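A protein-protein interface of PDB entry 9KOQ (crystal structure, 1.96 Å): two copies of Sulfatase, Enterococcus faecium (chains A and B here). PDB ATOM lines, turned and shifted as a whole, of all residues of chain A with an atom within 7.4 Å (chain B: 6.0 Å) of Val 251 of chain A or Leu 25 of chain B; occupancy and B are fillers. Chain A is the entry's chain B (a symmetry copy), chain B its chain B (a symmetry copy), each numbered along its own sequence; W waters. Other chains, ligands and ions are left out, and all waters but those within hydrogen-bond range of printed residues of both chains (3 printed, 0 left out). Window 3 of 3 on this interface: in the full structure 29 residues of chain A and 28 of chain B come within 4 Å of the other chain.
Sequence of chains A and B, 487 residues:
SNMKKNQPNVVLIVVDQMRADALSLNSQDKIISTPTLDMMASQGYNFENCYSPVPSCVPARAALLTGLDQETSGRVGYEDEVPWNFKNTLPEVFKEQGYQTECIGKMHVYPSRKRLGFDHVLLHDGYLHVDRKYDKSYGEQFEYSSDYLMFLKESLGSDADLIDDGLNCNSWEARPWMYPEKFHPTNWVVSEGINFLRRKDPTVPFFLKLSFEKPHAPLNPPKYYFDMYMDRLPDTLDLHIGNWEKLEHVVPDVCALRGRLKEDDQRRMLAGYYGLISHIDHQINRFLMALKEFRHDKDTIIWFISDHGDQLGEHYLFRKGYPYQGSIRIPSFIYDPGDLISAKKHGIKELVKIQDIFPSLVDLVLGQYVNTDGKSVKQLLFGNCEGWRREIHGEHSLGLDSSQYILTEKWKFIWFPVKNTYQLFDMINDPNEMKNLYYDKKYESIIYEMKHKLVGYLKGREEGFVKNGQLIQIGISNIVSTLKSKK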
ATOM      1  N   TRP A 172     -39.940 -24.991  13.155  1.00  0.00           N
ATOM      2  CA  TRP A 172     -39.318 -26.269  12.829  1.00  0.00           C
ATOM      3  C   TRP A 172     -38.909 -27.064  14.067  1.00  0.00           C
ATOM      4  O   TRP A 172     -38.495 -28.219  13.934  1.00  0.00           O
ATOM      5  CB  TRP A 172     -38.074 -26.037  11.961  1.00  0.00           C
ATOM      6  CG  TRP A 172     -37.231 -24.888  12.457  1.00  0.00           C
ATOM      7  CD1 TRP A 172     -37.315 -23.588  12.063  1.00  0.00           C
ATOM      8  CD2 TRP A 172     -36.191 -24.936  13.456  1.00  0.00           C
ATOM      9  NE1 TRP A 172     -36.396 -22.821  12.745  1.00  0.00           N
ATOM     10  CE2 TRP A 172     -35.691 -23.623  13.602  1.00  0.00           C
ATOM     11  CE3 TRP A 172     -35.639 -25.961  14.239  1.00  0.00           C
ATOM     12  CZ2 TRP A 172     -34.657 -23.303  14.493  1.00  0.00           C
ATOM     13  CZ3 TRP A 172     -34.613 -25.643  15.127  1.00  0.00           C
ATOM     14  CH2 TRP A 172     -34.138 -24.318  15.249  1.00  0.00           C
ATOM     15  N   GLU A 248     -28.275 -17.332   3.793  1.00  0.00           N
ATOM     16  CA  GLU A 248     -28.017 -16.058   4.453  1.00  0.00           C
ATOM     17  C   GLU A 248     -27.064 -16.189   5.639  1.00  0.00           C
ATOM     18  O   GLU A 248     -26.680 -15.165   6.215  1.00  0.00           O
ATOM     19  CB  GLU A 248     -29.352 -15.440   4.892  1.00  0.00           C
ATOM     20  CG  GLU A 248     -30.224 -15.029   3.687  1.00  0.00           C
ATOM     21  CD  GLU A 248     -31.608 -14.482   4.059  1.00  0.00           C
ATOM     22  OE1 GLU A 248     -32.011 -14.584   5.245  1.00  0.00           O
ATOM     23  OE2 GLU A 248     -32.302 -13.971   3.145  1.00  0.00           O
ATOM     24  N   HIS A 249     -26.688 -17.422   6.013  1.00  0.00           N
ATOM     25  CA  HIS A 249     -25.612 -17.708   6.973  1.00  0.00           C
ATOM     26  C   HIS A 249     -25.829 -17.028   8.322  1.00  0.00           C
ATOM     27  O   HIS A 249     -24.964 -16.318   8.842  1.00  0.00           O
ATOM     28  CB  HIS A 249     -24.250 -17.356   6.380  1.00  0.00           C
ATOM     29  CG  HIS A 249     -23.777 -18.361   5.378  1.00  0.00           C
ATOM     30  ND1 HIS A 249     -23.927 -18.189   4.018  1.00  0.00           N
ATOM     31  CD2 HIS A 249     -23.182 -19.568   5.541  1.00  0.00           C
ATOM     32  CE1 HIS A 249     -23.443 -19.245   3.387  1.00  0.00           C
ATOM     33  NE2 HIS A 249     -22.984 -20.096   4.288  1.00  0.00           N
ATOM     34  N   VAL A 250     -27.005 -17.274   8.900  1.00  0.00           N
ATOM     35  CA  VAL A 250     -27.361 -16.780  10.221  1.00  0.00           C
ATOM     36  C   VAL A 250     -27.981 -17.924  11.006  1.00  0.00           C
ATOM     37  O   VAL A 250     -28.455 -18.915  10.447  1.00  0.00           O
ATOM     38  CB  VAL A 250     -28.328 -15.574  10.171  1.00  0.00           C
ATOM     39  CG1 VAL A 250     -27.852 -14.539   9.166  1.00  0.00           C
ATOM     40  CG2 VAL A 250     -29.739 -16.035   9.817  1.00  0.00           C
ATOM     41  N   VAL A 251     -27.943 -17.778  12.326  1.00  0.00           N
ATOM     42  CA  VAL A 251     -28.701 -18.666  13.208  1.00  0.00           C
ATOM     43  C   VAL A 251     -30.176 -18.587  12.830  1.00  0.00           C
ATOM     44  O   VAL A 251     -30.734 -17.476  12.759  1.00  0.00           O
ATOM     45  CB  VAL A 251     -28.481 -18.261  14.679  1.00  0.00           C
ATOM     46  CG1 VAL A 251     -29.176 -19.222  15.603  1.00  0.00           C
ATOM     47  CG2 VAL A 251     -26.993 -18.212  14.990  1.00  0.00           C
ATOM     48  N   PRO A 252     -30.849 -19.704  12.559  1.00  0.00           N
ATOM     49  CA  PRO A 252     -32.244 -19.624  12.104  1.00  0.00           C
ATOM     50  C   PRO A 252     -33.167 -19.134  13.214  1.00  0.00           C
ATOM     51  O   PRO A 252     -33.093 -19.604  14.350  1.00  0.00           O
ATOM     52  CB  PRO A 252     -32.570 -21.071  11.694  1.00  0.00           C
ATOM     53  CG  PRO A 252     -31.622 -21.906  12.477  1.00  0.00           C
ATOM     54  CD  PRO A 252     -30.351 -21.087  12.575  1.00  0.00           C
ATOM     55  N   ASP A 253     -34.022 -18.160  12.877  1.00  0.00           N
ATOM     56  CA  ASP A 253     -35.175 -17.821  13.708  1.00  0.00           C
ATOM     57  C   ASP A 253     -35.957 -19.095  14.016  1.00  0.00           C
ATOM     58  O   ASP A 253     -36.056 -19.994  13.172  1.00  0.00           O
ATOM     59  CB  ASP A 253     -36.072 -16.816  12.958  1.00  0.00           C
ATOM     60  CG  ASP A 253     -37.134 -16.154  13.858  1.00  0.00           C
ATOM     61  OD1 ASP A 253     -38.123 -16.824  14.246  1.00  0.00           O
ATOM     62  OD2 ASP A 253     -37.026 -14.932  14.113  1.00  0.00           O
ATOM     63  N   VAL A 254     -36.510 -19.190  15.232  1.00  0.00           N
ATOM     64  CA  VAL A 254     -37.276 -20.397  15.542  1.00  0.00           C
ATOM     65  C   VAL A 254     -38.528 -20.510  14.665  1.00  0.00           C
ATOM     66  O   VAL A 254     -39.044 -21.615  14.487  1.00  0.00           O
ATOM     67  CB  VAL A 254     -37.625 -20.488  17.042  1.00  0.00           C
ATOM     68  CG1 VAL A 254     -36.359 -20.373  17.890  1.00  0.00           C
ATOM     69  CG2 VAL A 254     -38.609 -19.420  17.438  1.00  0.00           C
ATOM     70  N   ALA A 256     -38.435 -19.378  11.378  1.00  0.00           N
ATOM     71  CA  ALA A 256     -37.811 -18.923  10.138  1.00  0.00           C
ATOM     72  C   ALA A 256     -38.633 -19.289   8.904  1.00  0.00           C
ATOM     73  O   ALA A 256     -39.217 -20.377   8.823  1.00  0.00           O
ATOM     74  CB  ALA A 256     -36.418 -19.543  10.002  1.00  0.00           C
ATOM     75  N   ARG A 258     -36.817 -19.101   6.005  1.00  0.00           N
ATOM     76  CA  ARG A 258     -35.742 -19.596   5.161  1.00  0.00           C
ATOM     77  C   ARG A 258     -34.514 -19.823   6.043  1.00  0.00           C
ATOM     78  O   ARG A 258     -34.437 -19.312   7.163  1.00  0.00           O
ATOM     79  CB  ARG A 258     -35.476 -18.610   4.013  1.00  0.00           C
ATOM     80  CG  ARG A 258     -34.714 -17.366   4.393  1.00  0.00           C
ATOM     81  CD  ARG A 258     -34.431 -16.500   3.143  1.00  0.00           C
ATOM     82  NE  ARG A 258     -35.462 -16.552   2.107  1.00  0.00           N
ATOM     83  CZ  ARG A 258     -35.254 -16.836   0.826  1.00  0.00           C
ATOM     84  NH1 ARG A 258     -34.190 -17.516   0.431  1.00  0.00           N
ATOM     85  NH2 ARG A 258     -36.162 -16.471  -0.077  1.00  0.00           N
ATOM     86  N   GLY A 259     -33.576 -20.634   5.544  1.00  0.00           N
ATOM     87  CA  GLY A 259     -32.307 -20.892   6.185  1.00  0.00           C
ATOM     88  C   GLY A 259     -32.005 -22.377   6.242  1.00  0.00           C
ATOM     89  O   GLY A 259     -32.566 -23.181   5.489  1.00  0.00           O
ATOM     90  N   ARG A 260     -31.114 -22.751   7.155  1.00  0.00           N
ATOM     91  CA  ARG A 260     -30.640 -24.123   7.237  1.00  0.00           C
ATOM     92  C   ARG A 260     -30.475 -24.508   8.701  1.00  0.00           C
ATOM     93  O   ARG A 260     -29.981 -23.714   9.512  1.00  0.00           O
ATOM     94  CB  ARG A 260     -29.304 -24.298   6.493  1.00  0.00           C
ATOM     95  CG  ARG A 260     -28.659 -25.663   6.696  1.00  0.00           C
ATOM     96  CD  ARG A 260     -27.381 -25.805   5.887  1.00  0.00           C
ATOM     97  NE  ARG A 260     -26.367 -24.862   6.348  1.00  0.00           N
ATOM     98  CZ  ARG A 260     -25.229 -24.610   5.714  1.00  0.00           C
ATOM     99  NH1 ARG A 260     -24.893 -25.261   4.612  1.00  0.00           N
ATOM    100  NH2 ARG A 260     -24.414 -23.670   6.190  1.00  0.00           N
ATOM    101  N   LYS A 262     -29.226 -27.173  11.900  1.00  0.00           N
ATOM    102  CA  LYS A 262     -28.351 -28.267  12.307  1.00  0.00           C
ATOM    103  C   LYS A 262     -28.962 -29.583  11.852  1.00  0.00           C
ATOM    104  O   LYS A 262     -30.186 -29.724  11.791  1.00  0.00           O
ATOM    105  CB  LYS A 262     -28.165 -28.317  13.832  1.00  0.00           C
ATOM    106  CG  LYS A 262     -27.395 -27.173  14.480  1.00  0.00           C
ATOM    107  CD  LYS A 262     -27.426 -27.380  15.996  1.00  0.00           C
ATOM    108  CE  LYS A 262     -26.760 -26.267  16.768  1.00  0.00           C
ATOM    109  NZ  LYS A 262     -26.868 -26.514  18.247  1.00  0.00           N
ATOM    110  N   LEU B  23     -24.453 -22.325  26.014  1.00  0.00           N
ATOM    111  CA  LEU B  23     -25.274 -21.697  24.995  1.00  0.00           C
ATOM    112  C   LEU B  23     -24.671 -22.114  23.655  1.00  0.00           C
ATOM    113  O   LEU B  23     -23.469 -21.922  23.429  1.00  0.00           O
ATOM    114  CB  LEU B  23     -25.295 -20.176  25.168  1.00  0.00           C
ATOM    115  CG  LEU B  23     -25.873 -19.381  23.995  1.00  0.00           C
ATOM    116  CD1 LEU B  23     -27.373 -19.647  23.954  1.00  0.00           C
ATOM    117  CD2 LEU B  23     -25.611 -17.881  24.118  1.00  0.00           C
ATOM    118  N   SER B  24     -25.472 -22.757  22.802  1.00  0.00           N
ATOM    119  CA  SER B  24     -24.918 -23.299  21.561  1.00  0.00           C
ATOM    120  C   SER B  24     -24.168 -22.237  20.769  1.00  0.00           C
ATOM    121  O   SER B  24     -23.094 -22.506  20.221  1.00  0.00           O
ATOM    122  CB  SER B  24     -26.010 -23.917  20.689  1.00  0.00           C
ATOM    123  OG  SER B  24     -25.423 -24.815  19.750  1.00  0.00           O
ATOM    124  N   LEU B  25     -24.729 -21.027  20.702  1.00  0.00           N
ATOM    125  CA  LEU B  25     -24.103 -19.927  19.968  1.00  0.00           C
ATOM    126  C   LEU B  25     -22.669 -19.669  20.432  1.00  0.00           C
ATOM    127  O   LEU B  25     -21.793 -19.397  19.608  1.00  0.00           O
ATOM    128  CB  LEU B  25     -24.941 -18.659  20.131  1.00  0.00           C
ATOM    129  CG  LEU B  25     -24.459 -17.446  19.332  1.00  0.00           C
ATOM    130  CD1 LEU B  25     -24.687 -17.731  17.854  1.00  0.00           C
ATOM    131  CD2 LEU B  25     -25.178 -16.175  19.758  1.00  0.00           C
ATOM    132  N   ASN B  26     -22.420 -19.710  21.749  1.00  0.00           N
ATOM    133  CA  ASN B  26     -21.068 -19.594  22.297  1.00  0.00           C
ATOM    134  C   ASN B  26     -20.251 -20.869  22.181  1.00  0.00           C
ATOM    135  O   ASN B  26     -19.021 -20.807  22.253  1.00  0.00           O
ATOM    136  CB  ASN B  26     -21.100 -19.211  23.781  1.00  0.00           C
ATOM    137  CG  ASN B  26     -21.749 -17.875  24.037  1.00  0.00           C
ATOM    138  OD1 ASN B  26     -21.844 -17.043  23.145  1.00  0.00           O
ATOM    139  ND2 ASN B  26     -22.248 -17.684  25.260  1.00  0.00           N
ATOM    140  N   SER B  27     -20.892 -22.019  22.052  1.00  0.00           N
ATOM    141  CA  SER B  27     -20.159 -23.272  22.041  1.00  0.00           C
ATOM    142  C   SER B  27     -19.335 -23.402  20.767  1.00  0.00           C
ATOM    143  O   SER B  27     -19.620 -22.771  19.747  1.00  0.00           O
ATOM    144  CB  SER B  27     -21.127 -24.452  22.171  1.00  0.00           C
ATOM    145  OG  SER B  27     -21.530 -24.915  20.898  1.00  0.00           O
ATOM    146  N   LYS B  30     -21.206 -27.008  18.980  1.00  0.00           N
ATOM    147  CA  LYS B  30     -22.624 -26.837  18.617  1.00  0.00           C
ATOM    148  C   LYS B  30     -23.467 -28.074  18.916  1.00  0.00           C
ATOM    149  O   LYS B  30     -24.529 -28.268  18.301  1.00  0.00           O
ATOM    150  CB  LYS B  30     -22.807 -26.455  17.136  1.00  0.00           C
ATOM    151  CG  LYS B  30     -21.880 -25.356  16.620  1.00  0.00           C
ATOM    152  CD  LYS B  30     -22.079 -24.057  17.373  1.00  0.00           C
ATOM    153  CE  LYS B  30     -21.090 -22.997  16.905  1.00  0.00           C
ATOM    154  NZ  LYS B  30     -21.212 -21.761  17.727  1.00  0.00           N
ATOM    155  N   THR B  34     -29.926 -25.482  21.863  1.00  0.00           N
ATOM    156  CA  THR B  34     -30.573 -24.313  22.465  1.00  0.00           C
ATOM    157  C   THR B  34     -31.126 -23.394  21.370  1.00  0.00           C
ATOM    158  O   THR B  34     -30.726 -22.233  21.252  1.00  0.00           O
ATOM    159  CB  THR B  34     -29.603 -23.553  23.381  1.00  0.00           C
ATOM    160  OG1 THR B  34     -28.470 -23.097  22.626  1.00  0.00           O
ATOM    161  CG2 THR B  34     -29.114 -24.428  24.566  1.00  0.00           C
ATOM    162  N   PRO B  35     -32.079 -23.880  20.561  1.00  0.00           N
ATOM    163  CA  PRO B  35     -32.495 -23.087  19.385  1.00  0.00           C
ATOM    164  C   PRO B  35     -33.150 -21.766  19.735  1.00  0.00           C
ATOM    165  O   PRO B  35     -32.936 -20.773  19.028  1.00  0.00           O
ATOM    166  CB  PRO B  35     -33.470 -24.027  18.650  1.00  0.00           C
ATOM    167  CG  PRO B  35     -33.955 -24.977  19.714  1.00  0.00           C
ATOM    168  CD  PRO B  35     -32.783 -25.173  20.637  1.00  0.00           C
ATOM    169  N   LEU B  37     -32.717 -19.873  22.609  1.00  0.00           N
ATOM    170  CA  LEU B  37     -31.717 -18.960  23.155  1.00  0.00           C
ATOM    171  C   LEU B  37     -30.718 -18.530  22.083  1.00  0.00           C
ATOM    172  O   LEU B  37     -30.248 -17.387  22.095  1.00  0.00           O
ATOM    173  CB  LEU B  37     -30.993 -19.620  24.330  1.00  0.00           C
ATOM    174  CG  LEU B  37     -31.885 -19.966  25.543  1.00  0.00           C
ATOM    175  CD1 LEU B  37     -31.103 -20.739  26.611  1.00  0.00           C
ATOM    176  CD2 LEU B  37     -32.509 -18.708  26.126  1.00  0.00           C
ATOM    177  N   ASP B  38     -30.364 -19.441  21.168  1.00  0.00           N
ATOM    178  CA  ASP B  38     -29.510 -19.078  20.033  1.00  0.00           C
ATOM    179  C   ASP B  38     -30.104 -17.901  19.264  1.00  0.00           C
ATOM    180  O   ASP B  38     -29.423 -16.900  18.998  1.00  0.00           O
ATOM    181  CB  ASP B  38     -29.364 -20.273  19.089  1.00  0.00           C
ATOM    182  CG  ASP B  38     -28.249 -21.226  19.502  1.00  0.00           C
ATOM    183  OD1 ASP B  38     -27.655 -21.035  20.590  1.00  0.00           O
ATOM    184  OD2 ASP B  38     -27.994 -22.190  18.742  1.00  0.00           O
ATOM    185  N   MET B  39     -31.379 -18.019  18.888  1.00  0.00           N
ATOM    186  CA  MET B  39     -32.043 -16.966  18.132  1.00  0.00           C
ATOM    187  C   MET B  39     -32.052 -15.655  18.910  1.00  0.00           C
ATOM    188  O   MET B  39     -31.719 -14.597  18.370  1.00  0.00           O
ATOM    189  CB  MET B  39     -33.474 -17.393  17.789  1.00  0.00           C
ATOM    190  CG  MET B  39     -34.374 -16.207  17.406  1.00  0.00           C
ATOM    191  SD  MET B  39     -36.137 -16.577  17.242  1.00  0.00           S
ATOM    192  CE  MET B  39     -36.654 -16.550  18.956  1.00  0.00           C
ATOM    193  N   ALA B  41     -30.072 -14.627  21.381  1.00  0.00           N
ATOM    194  CA  ALA B  41     -28.744 -14.043  21.583  1.00  0.00           C
ATOM    195  C   ALA B  41     -28.174 -13.488  20.282  1.00  0.00           C
ATOM    196  O   ALA B  41     -27.538 -12.423  20.284  1.00  0.00           O
ATOM    197  CB  ALA B  41     -27.789 -15.084  22.166  1.00  0.00           C
ATOM    198  N   SER B  42     -28.364 -14.206  19.169  1.00  0.00           N
ATOM    199  CA  SER B  42     -27.820 -13.750  17.897  1.00  0.00           C
ATOM    200  C   SER B  42     -28.598 -12.575  17.338  1.00  0.00           C
ATOM    201  O   SER B  42     -28.029 -11.768  16.599  1.00  0.00           O
ATOM    202  CB  SER B  42     -27.792 -14.880  16.857  1.00  0.00           C
ATOM    203  OG  SER B  42     -29.100 -15.273  16.488  1.00  0.00           O
ATOM    204  N   GLN B  43     -29.878 -12.453  17.680  1.00  0.00           N
ATOM    205  CA  GLN B  43     -30.669 -11.334  17.205  1.00  0.00           C
ATOM    206  C   GLN B  43     -30.543 -10.105  18.091  1.00  0.00           C
ATOM    207  O   GLN B  43     -30.906  -9.011  17.657  1.00  0.00           O
ATOM    208  CB  GLN B  43     -32.147 -11.739  17.082  1.00  0.00           C
ATOM    209  CG  GLN B  43     -32.419 -12.634  15.866  1.00  0.00           C
ATOM    210  CD  GLN B  43     -33.872 -13.056  15.766  1.00  0.00           C
ATOM    211  OE1 GLN B  43     -34.703 -12.637  16.571  1.00  0.00           O
ATOM    212  NE2 GLN B  43     -34.185 -13.902  14.782  1.00  0.00           N
ATOM    213  N   ASN B  46     -25.238 -10.191  22.324  1.00  0.00           N
ATOM    214  CA  ASN B  46     -24.688 -11.321  23.054  1.00  0.00           C
ATOM    215  C   ASN B  46     -23.354 -10.920  23.673  1.00  0.00           C
ATOM    216  O   ASN B  46     -22.442 -10.491  22.959  1.00  0.00           O
ATOM    217  CB  ASN B  46     -24.496 -12.525  22.138  1.00  0.00           C
ATOM    218  CG  ASN B  46     -24.034 -13.742  22.900  1.00  0.00           C
ATOM    219  OD1 ASN B  46     -24.592 -14.062  23.951  1.00  0.00           O
ATOM    220  ND2 ASN B  46     -22.992 -14.407  22.407  1.00  0.00           N
HETATM  221  O   HOH W   1     -28.908 -24.831  19.157  1.00  0.00           O
HETATM  222  O   HOH W   2     -27.758 -29.474  18.601  1.00  0.00           O
HETATM  223  O   HOH W   3     -32.008 -21.120  16.492  1.00  0.00           O
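The side-chain carboxylate (OD2) of Asp 253 of chain A is in hydrogen-bond range of the side-chain amide nitrogen (NE2) of Gln 43 of chain B (3.1 Å). The backbone NH (N) of Val 254 of chain A sits at hydrogen-bond distance from the side-chain sulfur (SD) of Met 39 of chain B (3.3 Å). NZ of Lys 262 of chain A lies within hydrogen-bond range of OG of Ser 24 of chain B (2.7 Å). The side-chain amino group of Lys 262 of chain A sits at hydrogen-bond distance from the backbone carbonyl oxygen of Lys 30 of chain B (2.9 Å). SD of Met 39 of chain B lies close to OD1 of Asp 253 of chain A (3.6 Å).
The indole nitrogen of Trp 172 of chain A sits at hydrogen-bond distance from the backbone carbonyl oxygen of Asp 253 of chain A, at 2.9 Å. The backbone NH (N) of Ser 24 of chain B sits at hydrogen-bond distance from the side-chain hydroxyl (OG1) of Thr 34 of chain B, at 3.0 Å. The backbone carbonyl oxygen (O) of Leu 25 of chain B lies within hydrogen-bond range of the side-chain amino group (NZ) of Lys 30 of chain B, 3.1 Å away. The side-chain amino group of Lys 30 of chain B lies within hydrogen-bond range of the backbone carbonyl oxygen of Ser 27 of chain B, at 2.8 Å. O of Asp 38 of chain B is in hydrogen-bond range of OG of Ser 42 of chain B. O of Met 39 of chain B is in hydrogen-bond range of OG of Ser 42 of chain B, at 3.3 Å.
Among the printed residues, pairs that only touch across the chains: Trp 172 of chain A with Pro 35 of chain B (3.5 Å), Val 251 of chain A with Ser 42 of chain B (3.5 Å), Val 254 of chain A with Pro 35 of chain B (3.6 Å), Val 251 of chain A with Asp 38 of chain B (3.6 Å) and Val 251 of chain A with Leu 25 of chain B (3.7 Å).
Val 251 of chain A touches just these residues of chain B: Leu 25, Asp 38 and Ser 42. Of the printed residues of chain A, Ser 24 of chain B touches Lys 262 (2.7 Å). Of the printed residues of chain A, Pro 35 of chain B touches Trp 172 and Val 254. Ala 41 of chain B touches none of the printed residues of chain A. The nearest residue of chain A that does not touch Leu 25 of chain B is Lys 262 of chain A (6.4 Å).
Of the 13 printed residues of chain A, 5 touch a printed residue of chain B. Hydrophobic or aromatic side chains of chain A that line the printed part of chain B: Trp 172, Val 251 and Val 254. Hydrophobic or aromatic side chains of chain B that line the printed part of chain A: Leu 25, Pro 35 and Met 39. Among the printed residues, 10 pairs touch across the chains. Among the printed residues, no Asp or Glu carboxylate lies within 4 Å of a Lys or Arg side-chain nitrogen of the other chain.
No position is printed for both chains.
Water W3 lies within hydrogen-bond range of the backbone carbonyl oxygen (O) of Pro 35 of chain B (2.7 Å) and the backbone carbonyl oxygen (O) of Pro 252 of chain A (2.8 Å). Water W1 lies within hydrogen-bond range of the side-chain amino group of Lys 262 of chain A (2.8 Å), the side-chain carboxylate of Asp 38 of chain B (2.8 Å) and the backbone NH of Thr 34 of chain B (3.0 Å). Water W2 lies within hydrogen-bond range of the side-chain amino group of Lys 262 of chain A (3.1 Å) and the backbone carbonyl oxygen of Lys 30 of chain B (3.5 Å).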
